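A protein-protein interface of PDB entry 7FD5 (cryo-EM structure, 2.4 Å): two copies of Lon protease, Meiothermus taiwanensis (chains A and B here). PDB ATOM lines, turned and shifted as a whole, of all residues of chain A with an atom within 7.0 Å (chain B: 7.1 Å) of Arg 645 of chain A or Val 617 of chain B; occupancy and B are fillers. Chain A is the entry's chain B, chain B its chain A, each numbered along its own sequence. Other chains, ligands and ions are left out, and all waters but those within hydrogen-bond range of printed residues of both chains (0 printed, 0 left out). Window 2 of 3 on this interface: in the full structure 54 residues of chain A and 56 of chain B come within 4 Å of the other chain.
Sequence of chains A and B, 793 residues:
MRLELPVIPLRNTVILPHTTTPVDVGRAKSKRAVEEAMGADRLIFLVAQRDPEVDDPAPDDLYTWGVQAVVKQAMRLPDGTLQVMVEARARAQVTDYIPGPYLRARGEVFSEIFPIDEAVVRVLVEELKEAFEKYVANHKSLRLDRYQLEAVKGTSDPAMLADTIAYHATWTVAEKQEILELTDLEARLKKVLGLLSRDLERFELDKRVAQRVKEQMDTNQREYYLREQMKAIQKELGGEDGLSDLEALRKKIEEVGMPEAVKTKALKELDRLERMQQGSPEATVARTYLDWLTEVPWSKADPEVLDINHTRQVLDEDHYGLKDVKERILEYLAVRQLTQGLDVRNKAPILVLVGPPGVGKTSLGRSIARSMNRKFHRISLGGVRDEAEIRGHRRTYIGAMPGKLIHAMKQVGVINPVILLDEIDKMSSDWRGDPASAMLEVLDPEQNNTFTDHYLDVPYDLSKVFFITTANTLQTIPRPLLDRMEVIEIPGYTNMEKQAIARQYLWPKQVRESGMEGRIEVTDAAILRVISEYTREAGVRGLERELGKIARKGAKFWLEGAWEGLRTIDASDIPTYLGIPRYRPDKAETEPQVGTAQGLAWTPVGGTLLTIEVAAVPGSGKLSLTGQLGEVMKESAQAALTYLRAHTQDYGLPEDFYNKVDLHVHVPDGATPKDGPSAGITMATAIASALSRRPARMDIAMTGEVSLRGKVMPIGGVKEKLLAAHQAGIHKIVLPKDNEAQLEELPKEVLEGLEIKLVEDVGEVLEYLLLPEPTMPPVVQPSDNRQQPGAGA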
ATOM      1  N   ALA A 640      19.021  29.579   4.080  1.00  0.00           N
ATOM      2  CA  ALA A 640      19.975  28.482   3.938  1.00  0.00           C
ATOM      3  C   ALA A 640      19.331  27.248   3.326  1.00  0.00           C
ATOM      4  O   ALA A 640      19.939  26.576   2.485  1.00  0.00           O
ATOM      5  CB  ALA A 640      20.581  28.138   5.283  1.00  0.00           C
ATOM      6  N   LEU A 641      18.090  26.956   3.704  1.00  0.00           N
ATOM      7  CA  LEU A 641      17.408  25.810   3.117  1.00  0.00           C
ATOM      8  C   LEU A 641      17.100  26.011   1.642  1.00  0.00           C
ATOM      9  O   LEU A 641      17.192  25.061   0.862  1.00  0.00           O
ATOM     10  CB  LEU A 641      16.139  25.530   3.891  1.00  0.00           C
ATOM     11  CG  LEU A 641      15.315  24.343   3.457  1.00  0.00           C
ATOM     12  CD1 LEU A 641      16.097  23.105   3.624  1.00  0.00           C
ATOM     13  CD2 LEU A 641      14.109  24.308   4.301  1.00  0.00           C
ATOM     14  N   THR A 642      16.786  27.227   1.217  1.00  0.00           N
ATOM     15  CA  THR A 642      16.545  27.439  -0.204  1.00  0.00           C
ATOM     16  C   THR A 642      17.842  27.422  -0.996  1.00  0.00           C
ATOM     17  O   THR A 642      17.839  27.036  -2.163  1.00  0.00           O
ATOM     18  CB  THR A 642      15.786  28.738  -0.402  1.00  0.00           C
ATOM     19  OG1 THR A 642      14.613  28.692   0.400  1.00  0.00           O
ATOM     20  CG2 THR A 642      15.335  28.916  -1.810  1.00  0.00           C
ATOM     21  N   TYR A 643      18.959  27.808  -0.386  1.00  0.00           N
ATOM     22  CA  TYR A 643      20.241  27.574  -1.039  1.00  0.00           C
ATOM     23  C   TYR A 643      20.489  26.098  -1.259  1.00  0.00           C
ATOM     24  O   TYR A 643      20.945  25.698  -2.328  1.00  0.00           O
ATOM     25  CB  TYR A 643      21.386  28.156  -0.229  1.00  0.00           C
ATOM     26  CG  TYR A 643      22.721  27.807  -0.820  1.00  0.00           C
ATOM     27  CD1 TYR A 643      23.132  28.366  -2.004  1.00  0.00           C
ATOM     28  CD2 TYR A 643      23.566  26.919  -0.198  1.00  0.00           C
ATOM     29  CE1 TYR A 643      24.329  28.046  -2.547  1.00  0.00           C
ATOM     30  CE2 TYR A 643      24.763  26.594  -0.743  1.00  0.00           C
ATOM     31  CZ  TYR A 643      25.137  27.162  -1.911  1.00  0.00           C
ATOM     32  OH  TYR A 643      26.343  26.835  -2.449  1.00  0.00           O
ATOM     33  N   LEU A 644      20.193  25.271  -0.271  1.00  0.00           N
ATOM     34  CA  LEU A 644      20.489  23.854  -0.424  1.00  0.00           C
ATOM     35  C   LEU A 644      19.517  23.123  -1.327  1.00  0.00           C
ATOM     36  O   LEU A 644      19.881  22.082  -1.854  1.00  0.00           O
ATOM     37  CB  LEU A 644      20.507  23.167   0.928  1.00  0.00           C
ATOM     38  CG  LEU A 644      21.632  23.614   1.843  1.00  0.00           C
ATOM     39  CD1 LEU A 644      21.405  23.028   3.182  1.00  0.00           C
ATOM     40  CD2 LEU A 644      22.944  23.170   1.306  1.00  0.00           C
ATOM     41  N   ARG A 645      18.296  23.619  -1.518  1.00  0.00           N
ATOM     42  CA  ARG A 645      17.390  22.941  -2.445  1.00  0.00           C
ATOM     43  C   ARG A 645      17.798  23.101  -3.894  1.00  0.00           C
ATOM     44  O   ARG A 645      17.384  22.300  -4.726  1.00  0.00           O
ATOM     45  CB  ARG A 645      15.966  23.442  -2.290  1.00  0.00           C
ATOM     46  CG  ARG A 645      15.319  22.933  -1.077  1.00  0.00           C
ATOM     47  CD  ARG A 645      14.032  23.596  -0.773  1.00  0.00           C
ATOM     48  NE  ARG A 645      12.990  23.329  -1.736  1.00  0.00           N
ATOM     49  CZ  ARG A 645      11.795  23.883  -1.658  1.00  0.00           C
ATOM     50  NH1 ARG A 645      11.524  24.698  -0.665  1.00  0.00           N
ATOM     51  NH2 ARG A 645      10.871  23.616  -2.549  1.00  0.00           N
ATOM     52  N   ALA A 646      18.589  24.103  -4.215  1.00  0.00           N
ATOM     53  CA  ALA A 646      19.011  24.355  -5.576  1.00  0.00           C
ATOM     54  C   ALA A 646      20.360  23.757  -5.898  1.00  0.00           C
ATOM     55  O   ALA A 646      20.864  23.968  -6.995  1.00  0.00           O
ATOM     56  CB  ALA A 646      19.058  25.849  -5.833  1.00  0.00           C
ATOM     57  N   HIS A 647      20.965  23.039  -4.968  1.00  0.00           N
ATOM     58  CA  HIS A 647      22.267  22.430  -5.162  1.00  0.00           C
ATOM     59  C   HIS A 647      22.268  21.037  -4.572  1.00  0.00           C
ATOM     60  O   HIS A 647      23.190  20.648  -3.864  1.00  0.00           O
ATOM     61  CB  HIS A 647      23.368  23.265  -4.525  1.00  0.00           C
ATOM     62  CG  HIS A 647      23.564  24.593  -5.167  1.00  0.00           C
ATOM     63  ND1 HIS A 647      22.824  25.699  -4.824  1.00  0.00           N
ATOM     64  CD2 HIS A 647      24.426  25.000  -6.121  1.00  0.00           C
ATOM     65  CE1 HIS A 647      23.212  26.728  -5.549  1.00  0.00           C
ATOM     66  NE2 HIS A 647      24.186  26.331  -6.342  1.00  0.00           N
ATOM     67  N   THR A 648      21.222  20.267  -4.848  1.00  0.00           N
ATOM     68  CA  THR A 648      21.065  18.981  -4.190  1.00  0.00           C
ATOM     69  C   THR A 648      22.078  17.959  -4.641  1.00  0.00           C
ATOM     70  O   THR A 648      22.347  17.009  -3.907  1.00  0.00           O
ATOM     71  CB  THR A 648      19.688  18.406  -4.444  1.00  0.00           C
ATOM     72  OG1 THR A 648      19.515  18.228  -5.848  1.00  0.00           O
ATOM     73  CG2 THR A 648      18.649  19.323  -3.931  1.00  0.00           C
ATOM     74  N   GLN A 649      22.644  18.121  -5.820  1.00  0.00           N
ATOM     75  CA  GLN A 649      23.555  17.125  -6.335  1.00  0.00           C
ATOM     76  C   GLN A 649      25.005  17.463  -6.077  1.00  0.00           C
ATOM     77  O   GLN A 649      25.857  16.586  -6.213  1.00  0.00           O
ATOM     78  CB  GLN A 649      23.341  16.946  -7.827  1.00  0.00           C
ATOM     79  CG  GLN A 649      23.698  18.161  -8.609  1.00  0.00           C
ATOM     80  CD  GLN A 649      23.456  17.963 -10.075  1.00  0.00           C
ATOM     81  OE1 GLN A 649      23.027  16.892 -10.500  1.00  0.00           O
ATOM     82  NE2 GLN A 649      23.741  18.986 -10.868  1.00  0.00           N
ATOM     83  N   LEU A 653      22.909  15.559  -1.344  1.00  0.00           N
ATOM     84  CA  LEU A 653      21.643  15.583  -0.658  1.00  0.00           C
ATOM     85  C   LEU A 653      20.675  14.653  -1.378  1.00  0.00           C
ATOM     86  O   LEU A 653      20.876  14.345  -2.551  1.00  0.00           O
ATOM     87  CB  LEU A 653      21.120  17.011  -0.615  1.00  0.00           C
ATOM     88  CG  LEU A 653      22.081  17.962   0.086  1.00  0.00           C
ATOM     89  CD1 LEU A 653      21.552  19.354   0.107  1.00  0.00           C
ATOM     90  CD2 LEU A 653      22.350  17.514   1.464  1.00  0.00           C
ATOM     91  N   GLU A 655      17.332  13.441  -3.386  1.00  0.00           N
ATOM     92  CA  GLU A 655      16.880  14.126  -4.588  1.00  0.00           C
ATOM     93  C   GLU A 655      15.620  14.945  -4.346  1.00  0.00           C
ATOM     94  O   GLU A 655      15.505  16.066  -4.848  1.00  0.00           O
ATOM     95  CB  GLU A 655      16.651  13.124  -5.705  1.00  0.00           C
ATOM     96  CG  GLU A 655      16.379  13.790  -7.015  1.00  0.00           C
ATOM     97  CD  GLU A 655      17.593  14.522  -7.533  1.00  0.00           C
ATOM     98  OE1 GLU A 655      18.724  14.065  -7.268  1.00  0.00           O
ATOM     99  OE2 GLU A 655      17.424  15.565  -8.194  1.00  0.00           O
ATOM    100  N   PHE A 657      14.036  16.094  -1.053  1.00  0.00           N
ATOM    101  CA  PHE A 657      13.749  16.287   0.343  1.00  0.00           C
ATOM    102  C   PHE A 657      12.789  17.423   0.551  1.00  0.00           C
ATOM    103  O   PHE A 657      12.351  17.640   1.674  1.00  0.00           O
ATOM    104  CB  PHE A 657      15.029  16.514   1.137  1.00  0.00           C
ATOM    105  CG  PHE A 657      15.746  17.770   0.799  1.00  0.00           C
ATOM    106  CD1 PHE A 657      16.657  17.796  -0.220  1.00  0.00           C
ATOM    107  CD2 PHE A 657      15.550  18.909   1.536  1.00  0.00           C
ATOM    108  CE1 PHE A 657      17.317  18.933  -0.517  1.00  0.00           C
ATOM    109  CE2 PHE A 657      16.200  20.037   1.229  1.00  0.00           C
ATOM    110  CZ  PHE A 657      17.089  20.049   0.209  1.00  0.00           C
ATOM    111  N   TYR A 658      12.424  18.141  -0.505  1.00  0.00           N
ATOM    112  CA  TYR A 658      11.463  19.218  -0.342  1.00  0.00           C
ATOM    113  C   TYR A 658      10.061  18.695  -0.145  1.00  0.00           C
ATOM    114  O   TYR A 658       9.152  19.472   0.140  1.00  0.00           O
ATOM    115  CB  TYR A 658      11.494  20.145  -1.554  1.00  0.00           C
ATOM    116  CG  TYR A 658      10.937  19.578  -2.835  1.00  0.00           C
ATOM    117  CD1 TYR A 658      11.722  18.827  -3.677  1.00  0.00           C
ATOM    118  CD2 TYR A 658       9.636  19.848  -3.229  1.00  0.00           C
ATOM    119  CE1 TYR A 658      11.222  18.326  -4.844  1.00  0.00           C
ATOM    120  CE2 TYR A 658       9.131  19.347  -4.386  1.00  0.00           C
ATOM    121  CZ  TYR A 658       9.928  18.592  -5.191  1.00  0.00           C
ATOM    122  OH  TYR A 658       9.421  18.097  -6.357  1.00  0.00           O
ATOM    123  N   ASN A 659       9.881  17.404  -0.277  1.00  0.00           N
ATOM    124  CA  ASN A 659       8.600  16.791  -0.466  1.00  0.00           C
ATOM    125  C   ASN A 659       8.402  15.603   0.441  1.00  0.00           C
ATOM    126  O   ASN A 659       7.259  15.241   0.704  1.00  0.00           O
ATOM    127  CB  ASN A 659       8.493  16.343  -1.922  1.00  0.00           C
ATOM    128  CG  ASN A 659       7.113  16.241  -2.391  1.00  0.00           C
ATOM    129  OD1 ASN A 659       6.177  16.492  -1.653  1.00  0.00           O
ATOM    130  ND2 ASN A 659       6.958  15.890  -3.650  1.00  0.00           N
ATOM    131  N   ALA B 615      15.381  32.994  -6.243  1.00  0.00           N
ATOM    132  CA  ALA B 615      15.745  31.605  -6.612  1.00  0.00           C
ATOM    133  C   ALA B 615      14.496  30.841  -7.066  1.00  0.00           C
ATOM    134  O   ALA B 615      13.394  31.189  -6.597  1.00  0.00           O
ATOM    135  CB  ALA B 615      16.412  30.919  -5.446  1.00  0.00           C
ATOM    136  N   ALA B 616      14.665  29.840  -7.939  1.00  0.00           N
ATOM    137  CA  ALA B 616      13.541  29.048  -8.413  1.00  0.00           C
ATOM    138  C   ALA B 616      13.893  27.580  -8.314  1.00  0.00           C
ATOM    139  O   ALA B 616      14.813  27.110  -8.984  1.00  0.00           O
ATOM    140  CB  ALA B 616      13.164  29.407  -9.842  1.00  0.00           C
ATOM    141  N   VAL B 617      13.150  26.863  -7.495  1.00  0.00           N
ATOM    142  CA  VAL B 617      13.428  25.478  -7.141  1.00  0.00           C
ATOM    143  C   VAL B 617      12.173  24.692  -7.474  1.00  0.00           C
ATOM    144  O   VAL B 617      11.106  25.289  -7.654  1.00  0.00           O
ATOM    145  CB  VAL B 617      13.818  25.348  -5.654  1.00  0.00           C
ATOM    146  CG1 VAL B 617      15.104  26.029  -5.415  1.00  0.00           C
ATOM    147  CG2 VAL B 617      12.801  26.015  -4.837  1.00  0.00           C
ATOM    148  N   PRO B 618      12.256  23.370  -7.605  1.00  0.00           N
ATOM    149  CA  PRO B 618      11.034  22.593  -7.790  1.00  0.00           C
ATOM    150  C   PRO B 618      10.142  22.664  -6.568  1.00  0.00           C
ATOM    151  O   PRO B 618      10.610  22.826  -5.447  1.00  0.00           O
ATOM    152  CB  PRO B 618      11.553  21.180  -8.002  1.00  0.00           C
ATOM    153  CG  PRO B 618      12.868  21.351  -8.502  1.00  0.00           C
ATOM    154  CD  PRO B 618      13.435  22.527  -7.838  1.00  0.00           C
ATOM    155  N   GLY B 619       8.845  22.556  -6.787  1.00  0.00           N
ATOM    156  CA  GLY B 619       7.928  22.777  -5.695  1.00  0.00           C
ATOM    157  C   GLY B 619       6.489  22.771  -6.134  1.00  0.00           C
ATOM    158  O   GLY B 619       6.171  22.220  -7.182  1.00  0.00           O
ATOM    159  N   SER B 620       5.613  23.395  -5.366  1.00  0.00           N
ATOM    160  CA  SER B 620       4.188  23.341  -5.629  1.00  0.00           C
ATOM    161  C   SER B 620       3.554  24.694  -5.879  1.00  0.00           C
ATOM    162  O   SER B 620       2.334  24.769  -6.010  1.00  0.00           O
ATOM    163  CB  SER B 620       3.469  22.684  -4.456  1.00  0.00           C
ATOM    164  OG  SER B 620       3.593  23.498  -3.310  1.00  0.00           O
ATOM    165  N   GLY B 621       4.329  25.758  -5.903  1.00  0.00           N
ATOM    166  CA  GLY B 621       3.840  27.081  -6.199  1.00  0.00           C
ATOM    167  C   GLY B 621       3.646  27.834  -4.914  1.00  0.00           C
ATOM    168  O   GLY B 621       2.568  27.818  -4.335  1.00  0.00           O
ATOM    169  N   LYS B 622       4.673  28.549  -4.490  1.00  0.00           N
ATOM    170  CA  LYS B 622       4.642  29.320  -3.264  1.00  0.00           C
ATOM    171  C   LYS B 622       5.475  30.554  -3.496  1.00  0.00           C
ATOM    172  O   LYS B 622       6.117  30.702  -4.531  1.00  0.00           O
ATOM    173  CB  LYS B 622       5.193  28.564  -2.070  1.00  0.00           C
ATOM    174  CG  LYS B 622       4.335  27.467  -1.554  1.00  0.00           C
ATOM    175  CD  LYS B 622       4.980  26.843  -0.359  1.00  0.00           C
ATOM    176  CE  LYS B 622       4.080  25.799   0.252  1.00  0.00           C
ATOM    177  NZ  LYS B 622       3.891  24.652  -0.665  1.00  0.00           N
ATOM    178  N   LYS B 660       4.426  24.338 -10.268  1.00  0.00           N
ATOM    179  CA  LYS B 660       5.529  23.409 -10.313  1.00  0.00           C
ATOM    180  C   LYS B 660       6.815  23.997  -9.775  1.00  0.00           C
ATOM    181  O   LYS B 660       7.817  23.289  -9.721  1.00  0.00           O
ATOM    182  CB  LYS B 660       5.752  22.941 -11.742  1.00  0.00           C
ATOM    183  CG  LYS B 660       4.647  22.086 -12.255  1.00  0.00           C
ATOM    184  CD  LYS B 660       4.839  21.816 -13.722  1.00  0.00           C
ATOM    185  CE  LYS B 660       6.009  20.882 -13.966  1.00  0.00           C
ATOM    186  NZ  LYS B 660       5.736  19.504 -13.475  1.00  0.00           N
ATOM    187  N   VAL B 661       6.821  25.262  -9.383  1.00  0.00           N
ATOM    188  CA  VAL B 661       8.030  25.990  -9.036  1.00  0.00           C
ATOM    189  C   VAL B 661       7.746  26.793  -7.781  1.00  0.00           C
ATOM    190  O   VAL B 661       6.701  27.432  -7.688  1.00  0.00           O
ATOM    191  CB  VAL B 661       8.464  26.905 -10.198  1.00  0.00           C
ATOM    192  CG1 VAL B 661       9.476  27.887  -9.775  1.00  0.00           C
ATOM    193  CG2 VAL B 661       9.061  26.108 -11.296  1.00  0.00           C
ATOM    194  N   ASP B 662       8.651  26.748  -6.813  1.00  0.00           N
ATOM    195  CA  ASP B 662       8.626  27.665  -5.689  1.00  0.00           C
ATOM    196  C   ASP B 662       9.598  28.803  -5.924  1.00  0.00           C
ATOM    197  O   ASP B 662      10.680  28.600  -6.466  1.00  0.00           O
ATOM    198  CB  ASP B 662       8.998  26.962  -4.395  1.00  0.00           C
ATOM    199  CG  ASP B 662       7.922  26.042  -3.910  1.00  0.00           C
ATOM    200  OD1 ASP B 662       6.753  26.290  -4.226  1.00  0.00           O
ATOM    201  OD2 ASP B 662       8.224  25.071  -3.200  1.00  0.00           O
ATOM    202  N   LEU B 663       9.212  29.997  -5.507  1.00  0.00           N
ATOM    203  CA  LEU B 663      10.040  31.179  -5.629  1.00  0.00           C
ATOM    204  C   LEU B 663      10.399  31.697  -4.256  1.00  0.00           C
ATOM    205  O   LEU B 663       9.610  31.606  -3.325  1.00  0.00           O
ATOM    206  CB  LEU B 663       9.338  32.276  -6.401  1.00  0.00           C
ATOM    207  CG  LEU B 663       9.139  31.983  -7.866  1.00  0.00           C
ATOM    208  CD1 LEU B 663       8.292  33.036  -8.430  1.00  0.00           C
ATOM    209  CD2 LEU B 663      10.450  31.991  -8.538  1.00  0.00           C
ATOM    210  N   HIS B 664      11.595  32.236  -4.130  1.00  0.00           N
ATOM    211  CA  HIS B 664      12.035  32.812  -2.875  1.00  0.00           C
ATOM    212  C   HIS B 664      12.690  34.128  -3.216  1.00  0.00           C
ATOM    213  O   HIS B 664      13.766  34.130  -3.796  1.00  0.00           O
ATOM    214  CB  HIS B 664      13.016  31.903  -2.160  1.00  0.00           C
ATOM    215  CG  HIS B 664      13.239  32.262  -0.730  1.00  0.00           C
ATOM    216  ND1 HIS B 664      14.058  33.291  -0.338  1.00  0.00           N
ATOM    217  CD2 HIS B 664      12.798  31.689   0.406  1.00  0.00           C
ATOM    218  CE1 HIS B 664      14.085  33.358   0.975  1.00  0.00           C
ATOM    219  NE2 HIS B 664      13.325  32.398   1.452  1.00  0.00           N
ATOM    220  N   ARG B 693      16.268  31.438 -16.969  1.00  0.00           N
ATOM    221  CA  ARG B 693      17.672  31.031 -16.944  1.00  0.00           C
ATOM    222  C   ARG B 693      18.570  31.897 -17.813  1.00  0.00           C
ATOM    223  O   ARG B 693      19.677  31.494 -18.144  1.00  0.00           O
ATOM    224  CB  ARG B 693      17.819  29.564 -17.319  1.00  0.00           C
ATOM    225  CG  ARG B 693      17.173  28.673 -16.331  1.00  0.00           C
ATOM    226  CD  ARG B 693      18.027  28.651 -15.122  1.00  0.00           C
ATOM    227  NE  ARG B 693      17.564  27.720 -14.109  1.00  0.00           N
ATOM    228  CZ  ARG B 693      16.940  28.076 -12.997  1.00  0.00           C
ATOM    229  NH1 ARG B 693      16.733  29.351 -12.723  1.00  0.00           N
ATOM    230  NH2 ARG B 693      16.552  27.150 -12.138  1.00  0.00           N
ATOM    231  N   VAL B 779      14.868  24.469 -14.682  1.00  0.00           N
ATOM    232  CA  VAL B 779      14.058  23.613 -13.831  1.00  0.00           C
ATOM    233  C   VAL B 779      12.719  23.350 -14.510  1.00  0.00           C
ATOM    234  O   VAL B 779      12.080  24.264 -15.049  1.00  0.00           O
ATOM    235  CB  VAL B 779      13.905  24.243 -12.435  1.00  0.00           C
ATOM    236  CG1 VAL B 779      13.450  25.688 -12.524  1.00  0.00           C
ATOM    237  CG2 VAL B 779      12.927  23.461 -11.598  1.00  0.00           C
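The backbone carbonyl oxygen (O) of Pro 618 of chain B is in hydrogen-bond range of the guanidinium group (NH2) of Arg 645 of chain A (3.0 Å). OD2 of Asp 662 of chain B is in salt-bridge range of NH2 of Arg 645 of chain A (3.1 Å).
The backbone carbonyl oxygen (O) of His 664 of chain B is in hydrogen-bond range of the backbone NH (N) of Ala 615 of chain B (3.1 Å). The backbone NH of Asp 662 of chain B is in hydrogen-bond range of the backbone carbonyl oxygen of Val 617 of chain B (3.0 Å). O of Lys 660 of chain B sits at hydrogen-bond distance from N of Gly 619 of chain B (3.2 Å). N of Ser 620 of chain B sits at hydrogen-bond distance from OD1 of Asp 662 of chain B. The backbone NH (N) of Gly 621 of chain B is in hydrogen-bond range of the side-chain carboxylate (OD1) of Asp 662 of chain B (3.0 Å). The backbone NH (N) of Lys 622 of chain B lies within hydrogen-bond range of the side-chain carboxylate (OD1) of Asp 662 of chain B, at 3.1 Å.
Thr 642 of chain A touches His 664 of chain B. Val 617 of chain B touches Arg 645 of chain A (CG2 to NH2, 3.8 Å). Ala 646 of chain A touches Val 617 of chain B. Tyr 658 of chain A touches Pro 618 of chain B (CD2 to O, 3.8 Å). Tyr 658 of chain A touches Gly 619 of chain B.
Of chain B, only Val 617, Pro 618 and Asp 662 come within 4 Å of Arg 645 of chain A. Of the printed residues of chain A, Val 617 of chain B touches Arg 645 (3.8 Å) and Ala 646 (3.98 Å). Printed residues of chain A within 4 Å of Pro 618 of chain B: Arg 645 (3.0 Å) and Tyr 658 (3.8 Å). Of the printed residues of chain B, Thr 642 of chain A touches His 664. Printed residues of chain A within 4 Å of Gly 619 of chain B: Tyr 658. Of the printed residues of chain B, Tyr 658 of chain A touches Pro 618 and Gly 619. The nearest printed residue of chain A that does not touch Val 617 of chain B is Thr 642 of chain A (4.4 Å). The nearest printed residue of chain B that does not touch Ala 646 of chain A is Ala 616 of chain B (5.4 Å).
Of the 15 printed residues of chain B, 5 touch a printed residue of chain A.
No position is printed for both chains. Of the 7 pairs that touch across the chains among the printed residues, none has its exchanged pair printed and touching as well.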
